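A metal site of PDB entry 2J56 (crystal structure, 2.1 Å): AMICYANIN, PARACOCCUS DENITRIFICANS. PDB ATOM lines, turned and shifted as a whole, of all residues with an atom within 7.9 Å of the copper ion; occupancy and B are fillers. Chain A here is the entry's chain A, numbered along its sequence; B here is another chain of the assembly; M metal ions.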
ATOM      1  N   ILE A  25       9.637 -10.759 -19.689  1.00  0.00           N
ATOM      2  CA  ILE A  25       9.238  -9.619 -18.880  1.00  0.00           C
ATOM      3  C   ILE A  25       7.965  -9.080 -19.453  1.00  0.00           C
ATOM      4  O   ILE A  25       7.915  -8.708 -20.628  1.00  0.00           O
ATOM      5  CB  ILE A  25      10.318  -8.501 -18.859  1.00  0.00           C
ATOM      6  CG1 ILE A  25      11.709  -9.069 -18.572  1.00  0.00           C
ATOM      7  CG2 ILE A  25       9.924  -7.416 -17.828  1.00  0.00           C
ATOM      8  CD1 ILE A  25      12.841  -8.121 -19.006  1.00  0.00           C
ATOM      9  N   MET A  28       5.140  -5.566 -15.773  1.00  0.00           N
ATOM     10  CA  MET A  28       6.019  -5.077 -14.714  1.00  0.00           C
ATOM     11  C   MET A  28       6.504  -6.184 -13.773  1.00  0.00           C
ATOM     12  O   MET A  28       6.665  -5.933 -12.573  1.00  0.00           O
ATOM     13  CB  MET A  28       5.340  -3.968 -13.877  1.00  0.00           C
ATOM     14  CG  MET A  28       4.646  -2.898 -14.647  1.00  0.00           C
ATOM     15  SD  MET A  28       5.782  -1.940 -15.637  1.00  0.00           S
ATOM     16  CE  MET A  28       6.767  -1.185 -14.315  1.00  0.00           C
ATOM     17  N   LYS A  29       6.738  -7.392 -14.319  1.00  0.00           N
ATOM     18  CA  LYS A  29       7.314  -8.512 -13.549  1.00  0.00           C
ATOM     19  C   LYS A  29       8.262  -9.358 -14.405  1.00  0.00           C
ATOM     20  O   LYS A  29       8.053  -9.507 -15.615  1.00  0.00           O
ATOM     21  CB  LYS A  29       6.241  -9.486 -13.021  1.00  0.00           C
ATOM     22  CG  LYS A  29       5.325  -9.000 -11.908  1.00  0.00           C
ATOM     23  CD  LYS A  29       4.035  -9.828 -11.924  1.00  0.00           C
ATOM     24  CE  LYS A  29       3.102  -9.481 -10.778  1.00  0.00           C
ATOM     25  NZ  LYS A  29       3.238 -10.468  -9.629  1.00  0.00           N
ATOM     26  N   TYR A  30       9.281  -9.905 -13.753  1.00  0.00           N
ATOM     27  CA  TYR A  30      10.053 -10.982 -14.298  1.00  0.00           C
ATOM     28  C   TYR A  30       9.184 -12.238 -14.112  1.00  0.00           C
ATOM     29  O   TYR A  30       8.827 -12.587 -12.968  1.00  0.00           O
ATOM     30  CB  TYR A  30      11.402 -11.129 -13.595  1.00  0.00           C
ATOM     31  CG  TYR A  30      12.307  -9.912 -13.661  1.00  0.00           C
ATOM     32  CD1 TYR A  30      12.840  -9.484 -14.874  1.00  0.00           C
ATOM     33  CD2 TYR A  30      12.616  -9.188 -12.499  1.00  0.00           C
ATOM     34  CE1 TYR A  30      13.684  -8.339 -14.939  1.00  0.00           C
ATOM     35  CE2 TYR A  30      13.456  -8.059 -12.548  1.00  0.00           C
ATOM     36  CZ  TYR A  30      13.983  -7.636 -13.768  1.00  0.00           C
ATOM     37  OH  TYR A  30      14.825  -6.533 -13.843  1.00  0.00           O
ATOM     38  N   ASN A  47      12.108  -8.623 -23.143  1.00  0.00           N
ATOM     39  CA  ASN A  47      11.010  -7.715 -22.817  1.00  0.00           C
ATOM     40  C   ASN A  47       9.841  -7.918 -23.771  1.00  0.00           C
ATOM     41  O   ASN A  47       9.974  -7.800 -25.019  1.00  0.00           O
ATOM     42  CB  ASN A  47      11.478  -6.259 -22.802  1.00  0.00           C
ATOM     43  CG  ASN A  47      10.445  -5.316 -22.209  1.00  0.00           C
ATOM     44  OD1 ASN A  47       9.345  -5.727 -21.860  1.00  0.00           O
ATOM     45  ND2 ASN A  47      10.810  -4.029 -22.082  1.00  0.00           N
ATOM     46  N   GLU A  49       6.975  -6.052 -23.366  1.00  0.00           N
ATOM     47  CA  GLU A  49       6.121  -4.853 -23.395  1.00  0.00           C
ATOM     48  C   GLU A  49       6.786  -3.550 -23.860  1.00  0.00           C
ATOM     49  O   GLU A  49       8.022  -3.474 -23.967  1.00  0.00           O
ATOM     50  CB  GLU A  49       5.387  -4.646 -22.061  1.00  0.00           C
ATOM     51  CG  GLU A  49       6.281  -4.651 -20.822  1.00  0.00           C
ATOM     52  CD  GLU A  49       5.471  -4.731 -19.503  1.00  0.00           C
ATOM     53  OE1 GLU A  49       4.245  -4.959 -19.573  1.00  0.00           O
ATOM     54  OE2 GLU A  49       6.041  -4.586 -18.389  1.00  0.00           O
ATOM     55  N   MET A  51       6.872  -0.841 -22.228  1.00  0.00           N
ATOM     56  CA  MET A  51       7.618  -0.300 -21.055  1.00  0.00           C
ATOM     57  C   MET A  51       9.049  -0.835 -21.100  1.00  0.00           C
ATOM     58  O   MET A  51       9.240  -2.030 -21.060  1.00  0.00           O
ATOM     59  CB  MET A  51       6.945  -0.753 -19.753  1.00  0.00           C
ATOM     60  CG  MET A  51       7.728  -0.350 -18.487  1.00  0.00           C
ATOM     61  SD  MET A  51       7.487   1.413 -18.160  1.00  0.00           S
ATOM     62  CE  MET A  51       5.722   1.415 -17.755  1.00  0.00           C
ATOM     63  N   PRO A  52      10.062   0.051 -21.221  1.00  0.00           N
ATOM     64  CA  PRO A  52      11.454  -0.458 -21.132  1.00  0.00           C
ATOM     65  C   PRO A  52      11.802  -1.089 -19.786  1.00  0.00           C
ATOM     66  O   PRO A  52      11.377  -0.577 -18.749  1.00  0.00           O
ATOM     67  CB  PRO A  52      12.294   0.793 -21.413  1.00  0.00           C
ATOM     68  CG  PRO A  52      11.370   1.644 -22.246  1.00  0.00           C
ATOM     69  CD  PRO A  52      10.051   1.481 -21.548  1.00  0.00           C
ATOM     70  N   HIS A  53      12.510  -2.222 -19.811  1.00  0.00           N
ATOM     71  CA  HIS A  53      13.082  -2.852 -18.604  1.00  0.00           C
ATOM     72  C   HIS A  53      14.515  -3.336 -18.842  1.00  0.00           C
ATOM     73  O   HIS A  53      14.932  -3.541 -19.978  1.00  0.00           O
ATOM     74  CB  HIS A  53      12.310  -4.056 -18.054  1.00  0.00           C
ATOM     75  CG  HIS A  53      10.828  -3.893 -18.054  1.00  0.00           C
ATOM     76  ND1 HIS A  53      10.135  -3.413 -16.952  1.00  0.00           N
ATOM     77  CD2 HIS A  53       9.897  -4.198 -18.987  1.00  0.00           C
ATOM     78  CE1 HIS A  53       8.845  -3.426 -17.214  1.00  0.00           C
ATOM     79  NE2 HIS A  53       8.671  -3.891 -18.448  1.00  0.00           N
ATOM     80  N   ASN A  54      15.246  -3.540 -17.753  1.00  0.00           N
ATOM     81  CA  ASN A  54      16.548  -4.202 -17.864  1.00  0.00           C
ATOM     82  C   ASN A  54      16.714  -5.219 -16.716  1.00  0.00           C
ATOM     83  O   ASN A  54      15.757  -5.462 -15.966  1.00  0.00           O
ATOM     84  CB  ASN A  54      17.668  -3.143 -17.875  1.00  0.00           C
ATOM     85  CG  ASN A  54      17.922  -2.553 -16.503  1.00  0.00           C
ATOM     86  OD1 ASN A  54      17.046  -2.610 -15.632  1.00  0.00           O
ATOM     87  ND2 ASN A  54      19.139  -2.009 -16.281  1.00  0.00           N
ATOM     88  N   VAL A  55      17.936  -5.770 -16.576  1.00  0.00           N
ATOM     89  CA  VAL A  55      18.326  -6.445 -15.337  1.00  0.00           C
ATOM     90  C   VAL A  55      19.515  -5.714 -14.738  1.00  0.00           C
ATOM     91  O   VAL A  55      20.352  -5.171 -15.459  1.00  0.00           O
ATOM     92  CB  VAL A  55      18.658  -7.979 -15.555  1.00  0.00           C
ATOM     93  CG1 VAL A  55      17.388  -8.748 -16.011  1.00  0.00           C
ATOM     94  CG2 VAL A  55      19.771  -8.160 -16.570  1.00  0.00           C
ATOM     95  N   MET A  71      18.648  -1.159 -21.180  1.00  0.00           N
ATOM     96  CA  MET A  71      17.187  -1.212 -21.269  1.00  0.00           C
ATOM     97  C   MET A  71      16.763  -1.886 -22.542  1.00  0.00           C
ATOM     98  O   MET A  71      17.240  -1.560 -23.629  1.00  0.00           O
ATOM     99  CB  MET A  71      16.560   0.201 -21.183  1.00  0.00           C
ATOM    100  CG  MET A  71      16.941   0.954 -19.922  1.00  0.00           C
ATOM    101  SD  MET A  71      16.522   0.182 -18.335  1.00  0.00           S
ATOM    102  CE  MET A  71      14.743   0.260 -18.388  1.00  0.00           C
ATOM    103  N   HIS A  91      17.455  -6.632 -10.127  1.00  0.00           N
ATOM    104  CA  HIS A  91      16.223  -5.854 -10.165  1.00  0.00           C
ATOM    105  C   HIS A  91      16.199  -5.079 -11.450  1.00  0.00           C
ATOM    106  O   HIS A  91      17.155  -5.187 -12.228  1.00  0.00           O
ATOM    107  CB  HIS A  91      16.129  -4.924  -8.970  1.00  0.00           C
ATOM    108  CG  HIS A  91      17.108  -3.795  -9.012  1.00  0.00           C
ATOM    109  ND1 HIS A  91      18.403  -3.934  -8.589  1.00  0.00           N
ATOM    110  CD2 HIS A  91      16.972  -2.509  -9.411  1.00  0.00           C
ATOM    111  CE1 HIS A  91      19.039  -2.784  -8.729  1.00  0.00           C
ATOM    112  NE2 HIS A  91      18.189  -1.902  -9.223  1.00  0.00           N
ATOM    113  N   CYS A  92      15.116  -4.331 -11.709  1.00  0.00           N
ATOM    114  CA  CYS A  92      15.021  -3.463 -12.873  1.00  0.00           C
ATOM    115  C   CYS A  92      15.403  -2.033 -12.418  1.00  0.00           C
ATOM    116  O   CYS A  92      14.777  -1.497 -11.522  1.00  0.00           O
ATOM    117  CB  CYS A  92      13.585  -3.500 -13.436  1.00  0.00           C
ATOM    118  SG  CYS A  92      13.384  -2.593 -14.967  1.00  0.00           S
ATOM    119  N   THR A  93      16.433  -1.451 -13.026  1.00  0.00           N
ATOM    120  CA  THR A  93      16.960  -0.133 -12.632  1.00  0.00           C
ATOM    121  C   THR A  93      15.837   0.909 -12.254  1.00  0.00           C
ATOM    122  O   THR A  93      15.731   1.285 -11.085  1.00  0.00           O
ATOM    123  CB  THR A  93      17.921   0.410 -13.713  1.00  0.00           C
ATOM    124  OG1 THR A  93      19.052  -0.465 -13.818  1.00  0.00           O
ATOM    125  CG2 THR A  93      18.431   1.804 -13.365  1.00  0.00           C
ATOM    126  N   PRO A  94      14.950   1.302 -13.228  1.00  0.00           N
ATOM    127  CA  PRO A  94      13.901   2.299 -12.892  1.00  0.00           C
ATOM    128  C   PRO A  94      12.777   1.742 -12.030  1.00  0.00           C
ATOM    129  O   PRO A  94      11.943   2.517 -11.529  1.00  0.00           O
ATOM    130  CB  PRO A  94      13.335   2.682 -14.273  1.00  0.00           C
ATOM    131  CG  PRO A  94      13.508   1.345 -15.090  1.00  0.00           C
ATOM    132  CD  PRO A  94      14.848   0.837 -14.626  1.00  0.00           C
ATOM    133  N   HIS A  95      12.742   0.423 -11.858  1.00  0.00           N
ATOM    134  CA  HIS A  95      11.573  -0.267 -11.278  1.00  0.00           C
ATOM    135  C   HIS A  95      12.071  -1.256 -10.244  1.00  0.00           C
ATOM    136  O   HIS A  95      12.062  -2.501 -10.470  1.00  0.00           O
ATOM    137  CB  HIS A  95      10.714  -0.986 -12.370  1.00  0.00           C
ATOM    138  CG  HIS A  95      10.361  -0.136 -13.550  1.00  0.00           C
ATOM    139  ND1 HIS A  95      10.363  -0.611 -14.845  1.00  0.00           N
ATOM    140  CD2 HIS A  95      10.003   1.174 -13.634  1.00  0.00           C
ATOM    141  CE1 HIS A  95      10.022   0.366 -15.680  1.00  0.00           C
ATOM    142  NE2 HIS A  95       9.812   1.461 -14.975  1.00  0.00           N
ATOM    143  N   PRO A  96      12.537  -0.736  -9.082  1.00  0.00           N
ATOM    144  CA  PRO A  96      13.215  -1.591  -8.089  1.00  0.00           C
ATOM    145  C   PRO A  96      12.297  -2.586  -7.416  1.00  0.00           C
ATOM    146  O   PRO A  96      12.781  -3.485  -6.698  1.00  0.00           O
ATOM    147  CB  PRO A  96      13.752  -0.593  -7.028  1.00  0.00           C
ATOM    148  CG  PRO A  96      13.523   0.788  -7.592  1.00  0.00           C
ATOM    149  CD  PRO A  96      12.463   0.679  -8.665  1.00  0.00           C
ATOM    150  N   PHE A  97      10.991  -2.417  -7.626  1.00  0.00           N
ATOM    151  CA  PHE A  97      10.012  -3.404  -7.135  1.00  0.00           C
ATOM    152  C   PHE A  97      10.029  -4.654  -8.045  1.00  0.00           C
ATOM    153  O   PHE A  97       9.502  -5.704  -7.664  1.00  0.00           O
ATOM    154  CB  PHE A  97       8.588  -2.794  -7.065  1.00  0.00           C
ATOM    155  CG  PHE A  97       8.162  -2.134  -8.355  1.00  0.00           C
ATOM    156  CD1 PHE A  97       7.492  -2.877  -9.340  1.00  0.00           C
ATOM    157  CD2 PHE A  97       8.490  -0.787  -8.607  1.00  0.00           C
ATOM    158  CE1 PHE A  97       7.151  -2.285 -10.555  1.00  0.00           C
ATOM    159  CE2 PHE A  97       8.158  -0.196  -9.828  1.00  0.00           C
ATOM    160  CZ  PHE A  97       7.465  -0.944 -10.792  1.00  0.00           C
ATOM    161  N   MET A  98      10.622  -4.537  -9.245  1.00  0.00           N
ATOM    162  CA  MET A  98      10.767  -5.720 -10.131  1.00  0.00           C
ATOM    163  C   MET A  98      12.060  -6.422  -9.734  1.00  0.00           C
ATOM    164  O   MET A  98      13.159  -5.870  -9.889  1.00  0.00           O
ATOM    165  CB  MET A  98      10.811  -5.310 -11.610  1.00  0.00           C
ATOM    166  CG  MET A  98       9.548  -4.671 -12.180  1.00  0.00           C
ATOM    167  SD  MET A  98       9.901  -4.012 -13.851  1.00  0.00           S
ATOM    168  CE  MET A  98       9.919  -5.616 -14.680  1.00  0.00           C
ATOM    169  N   GLU B 101       7.123   4.072 -12.363  1.00  0.00           N
ATOM    170  CA  GLU B 101       7.291   3.883 -13.836  1.00  0.00           C
ATOM    171  C   GLU B 101       6.659   5.029 -14.642  1.00  0.00           C
ATOM    172  O   GLU B 101       7.097   5.328 -15.798  1.00  0.00           O
ATOM    173  CB  GLU B 101       6.768   2.511 -14.282  1.00  0.00           C
ATOM    174  CG  GLU B 101       5.299   2.249 -14.125  1.00  0.00           C
ATOM    175  CD  GLU B 101       4.890   1.767 -12.730  1.00  0.00           C
ATOM    176  OE1 GLU B 101       5.635   1.983 -11.739  1.00  0.00           O
ATOM    177  OE2 GLU B 101       3.810   1.166 -12.625  1.00  0.00           O
HETATM  178 CU    CU M   1      11.248  -2.560 -15.358  1.00  0.00          CU
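O of Met 51 lies close to NE2 of His 53, at 3.3 Å.
NE2 of His 53 is in hydrogen-bond range of OE2 of Glu 49 (2.7 Å).
The backbone NH (N) of Cys 92 sits at hydrogen-bond distance from the side-chain hydroxyl (OH) of Tyr 30, 3.1 Å away.
N of Asn 54 lies close to SG of Cys 92 (3.5 Å).
The backbone NH (N) of His 53 lies close to the side-chain amide nitrogen (ND2) of Asn 47.
Residues that only touch the copper ion: Pro 52 (3.9 Å).
Of the 21 residues printed, 5 come within 4 Å of the copper ion.
The nearest printed residue that does not touch the copper ion is Pro 94 (4.5 Å).
The copper ion is bound by ND1 of His 53 (2.1 Å), SG of Cys 92 (2.2 Å), ND1 of His 95 (2.2 Å) and SD of Met 98 (2.5 Å).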
